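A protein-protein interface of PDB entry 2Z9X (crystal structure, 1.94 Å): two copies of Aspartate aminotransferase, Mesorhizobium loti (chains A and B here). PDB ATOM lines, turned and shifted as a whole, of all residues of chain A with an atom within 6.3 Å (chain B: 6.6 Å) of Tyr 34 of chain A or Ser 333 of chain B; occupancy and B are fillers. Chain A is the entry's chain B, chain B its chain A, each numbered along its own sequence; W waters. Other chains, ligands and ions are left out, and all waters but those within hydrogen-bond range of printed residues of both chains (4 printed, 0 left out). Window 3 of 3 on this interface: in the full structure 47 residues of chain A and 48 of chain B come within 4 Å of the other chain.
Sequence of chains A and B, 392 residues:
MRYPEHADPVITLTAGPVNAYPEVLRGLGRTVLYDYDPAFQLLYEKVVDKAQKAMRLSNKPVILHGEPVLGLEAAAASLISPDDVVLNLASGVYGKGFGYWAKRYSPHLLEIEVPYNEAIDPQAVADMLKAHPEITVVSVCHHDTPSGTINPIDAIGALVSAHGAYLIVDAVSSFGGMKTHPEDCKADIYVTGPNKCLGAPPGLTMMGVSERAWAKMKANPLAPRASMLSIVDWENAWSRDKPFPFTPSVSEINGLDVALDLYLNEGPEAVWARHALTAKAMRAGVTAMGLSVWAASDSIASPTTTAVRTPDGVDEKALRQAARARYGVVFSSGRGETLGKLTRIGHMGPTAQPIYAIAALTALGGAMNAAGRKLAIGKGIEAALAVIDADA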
ATOM      1  N   VAL A  32     -20.692   3.735 -25.292  1.00  0.00           N
ATOM      2  CA  VAL A  32     -20.309   3.399 -23.919  1.00  0.00           C
ATOM      3  C   VAL A  32     -19.385   2.193 -23.954  1.00  0.00           C
ATOM      4  O   VAL A  32     -19.814   1.074 -24.292  1.00  0.00           O
ATOM      5  CB  VAL A  32     -21.536   3.104 -23.026  1.00  0.00           C
ATOM      6  CG1 VAL A  32     -21.100   2.688 -21.614  1.00  0.00           C
ATOM      7  CG2 VAL A  32     -22.446   4.349 -22.962  1.00  0.00           C
ATOM      8  N   LEU A  33     -18.117   2.423 -23.618  1.00  0.00           N
ATOM      9  CA  LEU A  33     -17.147   1.341 -23.562  1.00  0.00           C
ATOM     10  C   LEU A  33     -17.239   0.607 -22.233  1.00  0.00           C
ATOM     11  O   LEU A  33     -17.663   1.180 -21.217  1.00  0.00           O
ATOM     12  CB  LEU A  33     -15.710   1.864 -23.762  1.00  0.00           C
ATOM     13  CG  LEU A  33     -15.350   2.463 -25.140  1.00  0.00           C
ATOM     14  CD1 LEU A  33     -13.904   2.955 -25.162  1.00  0.00           C
ATOM     15  CD2 LEU A  33     -15.585   1.470 -26.278  1.00  0.00           C
ATOM     16  N   TYR A  34     -16.859  -0.666 -22.252  1.00  0.00           N
ATOM     17  CA  TYR A  34     -16.530  -1.403 -21.033  1.00  0.00           C
ATOM     18  C   TYR A  34     -15.486  -0.587 -20.274  1.00  0.00           C
ATOM     19  O   TYR A  34     -14.532  -0.095 -20.892  1.00  0.00           O
ATOM     20  CB  TYR A  34     -15.887  -2.719 -21.452  1.00  0.00           C
ATOM     21  CG  TYR A  34     -15.506  -3.717 -20.364  1.00  0.00           C
ATOM     22  CD1 TYR A  34     -14.339  -4.473 -20.510  1.00  0.00           C
ATOM     23  CD2 TYR A  34     -16.342  -3.978 -19.259  1.00  0.00           C
ATOM     24  CE1 TYR A  34     -13.990  -5.443 -19.588  1.00  0.00           C
ATOM     25  CE2 TYR A  34     -15.969  -4.949 -18.288  1.00  0.00           C
ATOM     26  CZ  TYR A  34     -14.797  -5.667 -18.487  1.00  0.00           C
ATOM     27  OH  TYR A  34     -14.389  -6.618 -17.604  1.00  0.00           O
ATOM     28  N   ASP A  35     -15.619  -0.486 -18.952  1.00  0.00           N
ATOM     29  CA  ASP A  35     -14.681   0.371 -18.192  1.00  0.00           C
ATOM     30  C   ASP A  35     -13.278  -0.198 -18.088  1.00  0.00           C
ATOM     31  O   ASP A  35     -12.319   0.541 -17.819  1.00  0.00           O
ATOM     32  CB  ASP A  35     -15.235   0.803 -16.807  1.00  0.00           C
ATOM     33  CG  ASP A  35     -15.747  -0.359 -15.959  1.00  0.00           C
ATOM     34  OD1 ASP A  35     -15.870  -1.487 -16.461  1.00  0.00           O
ATOM     35  OD2 ASP A  35     -16.022  -0.128 -14.758  1.00  0.00           O
ATOM     36  N   TYR A  36     -13.150  -1.507 -18.298  1.00  0.00           N
ATOM     37  CA  TYR A  36     -11.829  -2.131 -18.349  1.00  0.00           C
ATOM     38  C   TYR A  36     -11.274  -2.318 -19.754  1.00  0.00           C
ATOM     39  O   TYR A  36     -10.166  -2.846 -19.935  1.00  0.00           O
ATOM     40  CB  TYR A  36     -11.828  -3.437 -17.555  1.00  0.00           C
ATOM     41  CG  TYR A  36     -12.049  -3.168 -16.098  1.00  0.00           C
ATOM     42  CD1 TYR A  36     -13.329  -3.074 -15.570  1.00  0.00           C
ATOM     43  CD2 TYR A  36     -10.959  -2.947 -15.244  1.00  0.00           C
ATOM     44  CE1 TYR A  36     -13.532  -2.798 -14.225  1.00  0.00           C
ATOM     45  CE2 TYR A  36     -11.156  -2.682 -13.902  1.00  0.00           C
ATOM     46  CZ  TYR A  36     -12.445  -2.610 -13.400  1.00  0.00           C
ATOM     47  OH  TYR A  36     -12.631  -2.317 -12.062  1.00  0.00           O
ATOM     48  N   ASP A  37     -12.015  -1.852 -20.747  1.00  0.00           N
ATOM     49  CA  ASP A  37     -11.464  -1.728 -22.092  1.00  0.00           C
ATOM     50  C   ASP A  37     -10.256  -0.780 -22.017  1.00  0.00           C
ATOM     51  O   ASP A  37     -10.333   0.272 -21.371  1.00  0.00           O
ATOM     52  CB  ASP A  37     -12.539  -1.209 -23.051  1.00  0.00           C
ATOM     53  CG  ASP A  37     -12.064  -1.138 -24.486  1.00  0.00           C
ATOM     54  OD1 ASP A  37     -11.231  -0.270 -24.800  1.00  0.00           O
ATOM     55  OD2 ASP A  37     -12.517  -1.960 -25.296  1.00  0.00           O
ATOM     56  N   PRO A  38      -9.122  -1.158 -22.655  1.00  0.00           N
ATOM     57  CA  PRO A  38      -7.915  -0.336 -22.551  1.00  0.00           C
ATOM     58  C   PRO A  38      -8.109   1.079 -23.052  1.00  0.00           C
ATOM     59  O   PRO A  38      -7.466   1.985 -22.525  1.00  0.00           O
ATOM     60  CB  PRO A  38      -6.881  -1.092 -23.412  1.00  0.00           C
ATOM     61  CG  PRO A  38      -7.683  -1.996 -24.299  1.00  0.00           C
ATOM     62  CD  PRO A  38      -8.884  -2.367 -23.468  1.00  0.00           C
ATOM     63  N   PHE A  40     -10.920   2.862 -22.775  1.00  0.00           N
ATOM     64  CA  PHE A  40     -11.593   3.628 -21.730  1.00  0.00           C
ATOM     65  C   PHE A  40     -10.649   3.915 -20.574  1.00  0.00           C
ATOM     66  O   PHE A  40     -10.667   5.020 -20.009  1.00  0.00           O
ATOM     67  CB  PHE A  40     -12.868   2.973 -21.159  1.00  0.00           C
ATOM     68  CG  PHE A  40     -13.565   3.875 -20.167  1.00  0.00           C
ATOM     69  CD1 PHE A  40     -13.387   3.698 -18.802  1.00  0.00           C
ATOM     70  CD2 PHE A  40     -14.309   4.968 -20.618  1.00  0.00           C
ATOM     71  CE1 PHE A  40     -13.996   4.556 -17.869  1.00  0.00           C
ATOM     72  CE2 PHE A  40     -14.912   5.856 -19.700  1.00  0.00           C
ATOM     73  CZ  PHE A  40     -14.763   5.647 -18.324  1.00  0.00           C
ATOM     74  N   GLN A  41      -9.832   2.931 -20.213  1.00  0.00           N
ATOM     75  CA  GLN A  41      -8.877   3.099 -19.104  1.00  0.00           C
ATOM     76  C   GLN A  41      -7.926   4.266 -19.410  1.00  0.00           C
ATOM     77  O   GLN A  41      -7.607   5.089 -18.540  1.00  0.00           O
ATOM     78  CB  GLN A  41      -8.085   1.807 -18.881  1.00  0.00           C
ATOM     79  CG  GLN A  41      -8.891   0.691 -18.174  1.00  0.00           C
ATOM     80  CD  GLN A  41      -8.945   0.870 -16.661  1.00  0.00           C
ATOM     81  OE1 GLN A  41      -9.119   1.987 -16.155  1.00  0.00           O
ATOM     82  NE2 GLN A  41      -8.784  -0.229 -15.931  1.00  0.00           N
ATOM     83  N   VAL A 250     -19.635   6.355 -17.208  1.00  0.00           N
ATOM     84  CA  VAL A 250     -18.905   6.399 -18.485  1.00  0.00           C
ATOM     85  C   VAL A 250     -19.317   7.550 -19.379  1.00  0.00           C
ATOM     86  O   VAL A 250     -18.461   8.255 -19.889  1.00  0.00           O
ATOM     87  CB  VAL A 250     -18.965   5.034 -19.262  1.00  0.00           C
ATOM     88  CG1 VAL A 250     -18.350   5.179 -20.671  1.00  0.00           C
ATOM     89  CG2 VAL A 250     -18.213   3.944 -18.459  1.00  0.00           C
ATOM     90  N   THR B  12     -18.367  -4.514 -28.528  1.00  0.00           N
ATOM     91  CA  THR B  12     -18.236  -4.719 -27.096  1.00  0.00           C
ATOM     92  C   THR B  12     -19.346  -5.669 -26.625  1.00  0.00           C
ATOM     93  O   THR B  12     -20.528  -5.357 -26.734  1.00  0.00           O
ATOM     94  CB  THR B  12     -18.323  -3.367 -26.339  1.00  0.00           C
ATOM     95  OG1 THR B  12     -17.290  -2.490 -26.798  1.00  0.00           O
ATOM     96  CG2 THR B  12     -18.178  -3.571 -24.820  1.00  0.00           C
ATOM     97  N   THR B  14     -19.591  -7.146 -23.398  1.00  0.00           N
ATOM     98  CA  THR B  14     -19.257  -7.205 -21.983  1.00  0.00           C
ATOM     99  C   THR B  14     -20.509  -7.377 -21.128  1.00  0.00           C
ATOM    100  O   THR B  14     -21.627  -7.322 -21.639  1.00  0.00           O
ATOM    101  CB  THR B  14     -18.471  -5.931 -21.575  1.00  0.00           C
ATOM    102  OG1 THR B  14     -19.191  -4.763 -22.010  1.00  0.00           O
ATOM    103  CG2 THR B  14     -17.119  -5.964 -22.245  1.00  0.00           C
ATOM    104  N   ALA B  15     -20.321  -7.579 -19.822  1.00  0.00           N
ATOM    105  CA  ALA B  15     -21.425  -7.895 -18.918  1.00  0.00           C
ATOM    106  C   ALA B  15     -21.688  -6.780 -17.899  1.00  0.00           C
ATOM    107  O   ALA B  15     -22.328  -7.012 -16.884  1.00  0.00           O
ATOM    108  CB  ALA B  15     -21.147  -9.245 -18.197  1.00  0.00           C
ATOM    109  N   GLY B  16     -21.185  -5.573 -18.164  1.00  0.00           N
ATOM    110  CA  GLY B  16     -21.482  -4.414 -17.315  1.00  0.00           C
ATOM    111  C   GLY B  16     -20.197  -3.655 -16.990  1.00  0.00           C
ATOM    112  O   GLY B  16     -19.313  -4.194 -16.331  1.00  0.00           O
ATOM    113  N   PRO B  17     -20.068  -2.404 -17.472  1.00  0.00           N
ATOM    114  CA  PRO B  17     -21.022  -1.690 -18.322  1.00  0.00           C
ATOM    115  C   PRO B  17     -21.174  -2.373 -19.683  1.00  0.00           C
ATOM    116  O   PRO B  17     -20.387  -3.266 -20.019  1.00  0.00           O
ATOM    117  CB  PRO B  17     -20.379  -0.304 -18.517  1.00  0.00           C
ATOM    118  CG  PRO B  17     -18.989  -0.405 -18.074  1.00  0.00           C
ATOM    119  CD  PRO B  17     -18.860  -1.605 -17.177  1.00  0.00           C
ATOM    120  N   VAL B  18     -22.177  -1.937 -20.447  1.00  0.00           N
ATOM    121  CA  VAL B  18     -22.446  -2.405 -21.810  1.00  0.00           C
ATOM    122  C   VAL B  18     -22.767  -1.181 -22.677  1.00  0.00           C
ATOM    123  O   VAL B  18     -23.090  -0.117 -22.141  1.00  0.00           O
ATOM    124  CB  VAL B  18     -23.692  -3.364 -21.857  1.00  0.00           C
ATOM    125  CG1 VAL B  18     -23.572  -4.501 -20.837  1.00  0.00           C
ATOM    126  CG2 VAL B  18     -25.005  -2.600 -21.615  1.00  0.00           C
ATOM    127  N   ASN B  19     -22.714  -1.310 -23.997  1.00  0.00           N
ATOM    128  CA  ASN B  19     -23.147  -0.195 -24.853  1.00  0.00           C
ATOM    129  C   ASN B  19     -24.618   0.083 -24.636  1.00  0.00           C
ATOM    130  O   ASN B  19     -25.423  -0.852 -24.412  1.00  0.00           O
ATOM    131  CB  ASN B  19     -22.895  -0.464 -26.338  1.00  0.00           C
ATOM    132  CG  ASN B  19     -22.929   0.825 -27.209  1.00  0.00           C
ATOM    133  OD1 ASN B  19     -23.013   0.735 -28.443  1.00  0.00           O
ATOM    134  ND2 ASN B  19     -22.826   2.010 -26.577  1.00  0.00           N
ATOM    135  N   PRO B 146     -20.607 -11.888 -12.035  1.00  0.00           N
ATOM    136  CA  PRO B 146     -19.260 -12.482 -12.208  1.00  0.00           C
ATOM    137  C   PRO B 146     -19.245 -14.012 -12.325  1.00  0.00           C
ATOM    138  O   PRO B 146     -18.213 -14.585 -12.671  1.00  0.00           O
ATOM    139  CB  PRO B 146     -18.505 -12.006 -10.955  1.00  0.00           C
ATOM    140  CG  PRO B 146     -19.222 -10.709 -10.563  1.00  0.00           C
ATOM    141  CD  PRO B 146     -20.675 -11.002 -10.850  1.00  0.00           C
ATOM    142  N   GLU B 316      -6.176 -16.136 -18.913  1.00  0.00           N
ATOM    143  CA  GLU B 316      -7.480 -15.539 -19.255  1.00  0.00           C
ATOM    144  C   GLU B 316      -7.373 -14.084 -19.685  1.00  0.00           C
ATOM    145  O   GLU B 316      -8.093 -13.646 -20.586  1.00  0.00           O
ATOM    146  CB  GLU B 316      -8.460 -15.655 -18.089  1.00  0.00           C
ATOM    147  CG  GLU B 316      -9.923 -15.479 -18.504  1.00  0.00           C
ATOM    148  CD  GLU B 316     -10.361 -14.019 -18.608  1.00  0.00           C
ATOM    149  OE1 GLU B 316      -9.804 -13.141 -17.902  1.00  0.00           O
ATOM    150  OE2 GLU B 316     -11.280 -13.755 -19.407  1.00  0.00           O
ATOM    151  N   ARG B 320      -8.464 -12.459 -23.366  1.00  0.00           N
ATOM    152  CA  ARG B 320      -9.284 -11.256 -23.670  1.00  0.00           C
ATOM    153  C   ARG B 320      -8.533 -10.224 -24.495  1.00  0.00           C
ATOM    154  O   ARG B 320      -9.110  -9.563 -25.372  1.00  0.00           O
ATOM    155  CB  ARG B 320      -9.835 -10.603 -22.402  1.00  0.00           C
ATOM    156  CG  ARG B 320     -11.028 -11.356 -21.831  1.00  0.00           C
ATOM    157  CD  ARG B 320     -11.557 -10.721 -20.551  1.00  0.00           C
ATOM    158  NE  ARG B 320     -10.612 -10.855 -19.446  1.00  0.00           N
ATOM    159  CZ  ARG B 320      -9.855  -9.852 -18.987  1.00  0.00           C
ATOM    160  NH1 ARG B 320      -9.025 -10.060 -17.970  1.00  0.00           N
ATOM    161  NH2 ARG B 320      -9.937  -8.635 -19.537  1.00  0.00           N
ATOM    162  N   VAL B 330     -14.662  -7.296 -27.557  1.00  0.00           N
ATOM    163  CA  VAL B 330     -14.323  -7.115 -26.140  1.00  0.00           C
ATOM    164  C   VAL B 330     -15.240  -7.963 -25.259  1.00  0.00           C
ATOM    165  O   VAL B 330     -16.456  -7.858 -25.352  1.00  0.00           O
ATOM    166  CB  VAL B 330     -14.473  -5.653 -25.691  1.00  0.00           C
ATOM    167  CG1 VAL B 330     -13.988  -5.492 -24.240  1.00  0.00           C
ATOM    168  CG2 VAL B 330     -13.663  -4.750 -26.638  1.00  0.00           C
ATOM    169  N   PHE B 331     -14.623  -8.765 -24.402  1.00  0.00           N
ATOM    170  CA  PHE B 331     -15.322  -9.562 -23.401  1.00  0.00           C
ATOM    171  C   PHE B 331     -15.029  -9.030 -21.996  1.00  0.00           C
ATOM    172  O   PHE B 331     -14.055  -8.297 -21.793  1.00  0.00           O
ATOM    173  CB  PHE B 331     -14.850 -11.015 -23.484  1.00  0.00           C
ATOM    174  CG  PHE B 331     -15.152 -11.677 -24.797  1.00  0.00           C
ATOM    175  CD1 PHE B 331     -16.408 -11.533 -25.402  1.00  0.00           C
ATOM    176  CD2 PHE B 331     -14.183 -12.441 -25.434  1.00  0.00           C
ATOM    177  CE1 PHE B 331     -16.695 -12.167 -26.613  1.00  0.00           C
ATOM    178  CE2 PHE B 331     -14.468 -13.074 -26.658  1.00  0.00           C
ATOM    179  CZ  PHE B 331     -15.719 -12.948 -27.230  1.00  0.00           C
ATOM    180  N   SER B 332     -15.864  -9.427 -21.033  1.00  0.00           N
ATOM    181  CA  SER B 332     -15.624  -9.128 -19.628  1.00  0.00           C
ATOM    182  C   SER B 332     -14.728 -10.171 -18.962  1.00  0.00           C
ATOM    183  O   SER B 332     -14.792 -11.383 -19.267  1.00  0.00           O
ATOM    184  CB  SER B 332     -16.942  -9.049 -18.852  1.00  0.00           C
ATOM    185  OG  SER B 332     -17.598  -7.809 -19.063  1.00  0.00           O
ATOM    186  N   SER B 333     -13.913  -9.695 -18.025  1.00  0.00           N
ATOM    187  CA  SER B 333     -13.204 -10.561 -17.108  1.00  0.00           C
ATOM    188  C   SER B 333     -14.195 -11.049 -16.065  1.00  0.00           C
ATOM    189  O   SER B 333     -15.351 -10.583 -16.031  1.00  0.00           O
ATOM    190  CB  SER B 333     -12.081  -9.769 -16.430  1.00  0.00           C
ATOM    191  OG  SER B 333     -12.585  -8.808 -15.524  1.00  0.00           O
ATOM    192  N   GLY B 334     -13.759 -11.981 -15.214  1.00  0.00           N
ATOM    193  CA  GLY B 334     -14.466 -12.261 -13.969  1.00  0.00           C
ATOM    194  C   GLY B 334     -14.271 -11.113 -12.990  1.00  0.00           C
ATOM    195  O   GLY B 334     -13.788 -10.031 -13.364  1.00  0.00           O
ATOM    196  N   ARG B 335     -14.632 -11.350 -11.732  1.00  0.00           N
ATOM    197  CA  ARG B 335     -14.508 -10.340 -10.672  1.00  0.00           C
ATOM    198  C   ARG B 335     -14.241 -11.094  -9.372  1.00  0.00           C
ATOM    199  O   ARG B 335     -14.802 -12.166  -9.153  1.00  0.00           O
ATOM    200  CB  ARG B 335     -15.797  -9.511 -10.579  1.00  0.00           C
ATOM    201  CG  ARG B 335     -15.762  -8.421  -9.529  1.00  0.00           C
ATOM    202  CD  ARG B 335     -16.986  -7.537  -9.535  1.00  0.00           C
ATOM    203  NE  ARG B 335     -16.822  -6.501  -8.510  1.00  0.00           N
ATOM    204  CZ  ARG B 335     -16.384  -5.268  -8.760  1.00  0.00           C
ATOM    205  NH1 ARG B 335     -16.107  -4.900 -10.001  1.00  0.00           N
ATOM    206  NH2 ARG B 335     -16.233  -4.399  -7.766  1.00  0.00           N
ATOM    207  N   THR B 338     -13.814 -15.057  -9.171  1.00  0.00           N
ATOM    208  CA  THR B 338     -13.853 -15.599 -10.550  1.00  0.00           C
ATOM    209  C   THR B 338     -12.866 -14.929 -11.517  1.00  0.00           C
ATOM    210  O   THR B 338     -12.709 -15.378 -12.649  1.00  0.00           O
ATOM    211  CB  THR B 338     -15.269 -15.579 -11.172  1.00  0.00           C
ATOM    212  OG1 THR B 338     -15.639 -14.238 -11.520  1.00  0.00           O
ATOM    213  CG2 THR B 338     -16.311 -16.185 -10.218  1.00  0.00           C
ATOM    214  N   LEU B 339     -12.204 -13.862 -11.074  1.00  0.00           N
ATOM    215  CA  LEU B 339     -11.203 -13.197 -11.904  1.00  0.00           C
ATOM    216  C   LEU B 339     -10.083 -14.182 -12.230  1.00  0.00           C
ATOM    217  O   LEU B 339      -9.497 -14.793 -11.341  1.00  0.00           O
ATOM    218  CB  LEU B 339     -10.642 -11.950 -11.211  1.00  0.00           C
ATOM    219  CG  LEU B 339      -9.626 -11.133 -12.017  1.00  0.00           C
ATOM    220  CD1 LEU B 339     -10.196 -10.657 -13.363  1.00  0.00           C
ATOM    221  CD2 LEU B 339      -9.135  -9.946 -11.188  1.00  0.00           C
ATOM    222  N   GLY B 340      -9.805 -14.335 -13.515  1.00  0.00           N
ATOM    223  CA  GLY B 340      -8.792 -15.255 -13.981  1.00  0.00           C
ATOM    224  C   GLY B 340      -9.299 -16.660 -14.235  1.00  0.00           C
ATOM    225  O   GLY B 340      -8.586 -17.473 -14.820  1.00  0.00           O
ATOM    226  N   LEU B 342     -12.638 -17.434 -15.495  1.00  0.00           N
ATOM    227  CA  LEU B 342     -13.681 -17.498 -16.520  1.00  0.00           C
ATOM    228  C   LEU B 342     -13.681 -16.212 -17.343  1.00  0.00           C
ATOM    229  O   LEU B 342     -13.098 -15.197 -16.926  1.00  0.00           O
ATOM    230  CB  LEU B 342     -15.050 -17.708 -15.865  1.00  0.00           C
ATOM    231  CG  LEU B 342     -15.576 -16.695 -14.825  1.00  0.00           C
ATOM    232  CD1 LEU B 342     -16.160 -15.421 -15.474  1.00  0.00           C
ATOM    233  CD2 LEU B 342     -16.636 -17.370 -13.949  1.00  0.00           C
ATOM    234  N   THR B 343     -14.350 -16.260 -18.495  1.00  0.00           N
ATOM    235  CA  THR B 343     -14.538 -15.088 -19.359  1.00  0.00           C
ATOM    236  C   THR B 343     -16.028 -14.896 -19.465  1.00  0.00           C
ATOM    237  O   THR B 343     -16.769 -15.890 -19.536  1.00  0.00           O
ATOM    238  CB  THR B 343     -13.948 -15.331 -20.775  1.00  0.00           C
ATOM    239  OG1 THR B 343     -12.560 -15.659 -20.645  1.00  0.00           O
ATOM    240  CG2 THR B 343     -14.089 -14.089 -21.648  1.00  0.00           C
ATOM    241  N   ARG B 344     -16.484 -13.641 -19.424  1.00  0.00           N
ATOM    242  CA  ARG B 344     -17.927 -13.366 -19.571  1.00  0.00           C
ATOM    243  C   ARG B 344     -18.265 -12.711 -20.900  1.00  0.00           C
ATOM    244  O   ARG B 344     -17.600 -11.752 -21.344  1.00  0.00           O
ATOM    245  CB  ARG B 344     -18.447 -12.494 -18.414  1.00  0.00           C
ATOM    246  CG  ARG B 344     -18.469 -13.211 -17.068  1.00  0.00           C
ATOM    247  CD  ARG B 344     -18.962 -12.284 -15.963  1.00  0.00           C
ATOM    248  NE  ARG B 344     -18.015 -11.214 -15.614  1.00  0.00           N
ATOM    249  CZ  ARG B 344     -18.320 -10.141 -14.879  1.00  0.00           C
ATOM    250  NH1 ARG B 344     -19.571  -9.928 -14.450  1.00  0.00           N
ATOM    251  NH2 ARG B 344     -17.374  -9.256 -14.594  1.00  0.00           N
HETATM  252  O   HOH W   1     -15.277  -2.154 -11.070  1.00  0.00           O
HETATM  253  O   HOH W   2     -16.916  -3.577 -15.160  1.00  0.00           O
HETATM  254  O   HOH W   3     -15.376  -1.901 -24.777  1.00  0.00           O
HETATM  255  O   HOH W   4      -9.830  -5.641 -20.204  1.00  0.00           O
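Water W2 lies within hydrogen-bond range of the side-chain carboxylate (OD1) of Asp 35 of chain A (2.7 Å) and the backbone carbonyl oxygen (O) of Gly 16 of chain B (2.7 Å).
Water W4 bridges O of Tyr 36 of chain A (2.8 Å) and NH2 of Arg 320 of chain B (3.1 Å).
Water W1 bridges the side-chain hydroxyl (OH) of Tyr 36 of chain A and the guanidinium group (NH1) of Arg 335 of chain B.
Water W3 lies within hydrogen-bond range of OG1 of Thr 12 of chain B (2.8 Å), OD2 of Asp 37 of chain A (2.9 Å) and N of Tyr 34 of chain A (3.2 Å).
OG1 of Thr 14 of chain B sits at hydrogen-bond distance from O of Pro 17 of chain B (2.8 Å).
The side-chain hydroxyl (OG) of Ser 332 of chain B is in hydrogen-bond range of the backbone NH (N) of Ala 15 of chain B, at 2.8 Å.
O of Ser 332 of chain B is in hydrogen-bond range of N of Arg 344 of chain B, at 2.8 Å.
The backbone carbonyl oxygen of Ser 333 of chain B lies within hydrogen-bond range of the guanidinium group of Arg 344 of chain B, 2.8 Å away.
The side-chain amide nitrogen (ND2) of Asn 19 of chain B lies close to the backbone NH (N) of Val 32 of chain A, 3.0 Å away.
The backbone NH of Ser 333 of chain B sits at hydrogen-bond distance from the side-chain hydroxyl of Tyr 34 of chain A (3.1 Å).
Printed residues of chain B that touch a printed residue of chain A: Thr 14, Gly 16, Pro 17, Val 18, Asn 19, Val 330, Phe 331, Ser 332 and Ser 333.
Hydrophobic or aromatic side chains of chain B within 4 Å of the printed part of chain A: Pro 17 and Val 330.
Among the printed residues, no Asp or Glu carboxylate lies within 4 Å of a Lys or Arg side-chain nitrogen of the other chain.
Tyr 34 of chain A touches seven residues of chain B.
Ser 333 of chain B touches just one residue of chain A: Tyr 34 (3.1 Å).
Of the printed residues of chain A, Phe 331 of chain B touches Tyr 34.
Printed residues of chain A within 4 Å of Pro 17 of chain B: Leu 33 (3.8 Å), Tyr 34 (3.97 Å) and Asp 35 (3.1 Å).
Printed residues of chain B within 4 Å of Val 32 of chain A: Val 18 (3.5 Å) and Asn 19 (3.0 Å).
Of the printed residues of chain A, Thr 14 of chain B touches Tyr 34.
Printed residues of chain A within 4 Å of Ser 332 of chain B: Tyr 34.
Glu 316 of chain B touches none of the printed residues of chain A.
The nearest residue of chain B that does not touch Tyr 34 of chain A is Thr 12 of chain B (4.1 Å).
The nearest printed residue of chain B that does not touch Asp 37 of chain A is Thr 12 of chain B (5.0 Å).
No position is printed for both chains.
Of the 12 pairs that touch across the chains among the printed residues, none has its exchanged pair printed and touching as well.
Among the printed residues, pairs that only touch across the chains: Asp 35 of chain A with Pro 17 of chain B (3.1 Å), Asp 37 of chain A with Val 330 of chain B (3.3 Å), Tyr 34 of chain A with Thr 14 of chain B (3.3 Å), Tyr 34 of chain A with Ser 332 of chain B (3.4 Å), Val 32 of chain A with Val 18 of chain B (3.5 Å), Tyr 34 of chain A with Phe 331 of chain B (3.6 Å), Leu 33 of chain A with Pro 17 of chain B (3.8 Å), Tyr 34 of chain A with Val 330 of chain B (3.9 Å), Tyr 34 of chain A with Gly 16 of chain B (3.9 Å) and Tyr 34 of chain A with Pro 17 of chain B (3.97 Å).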
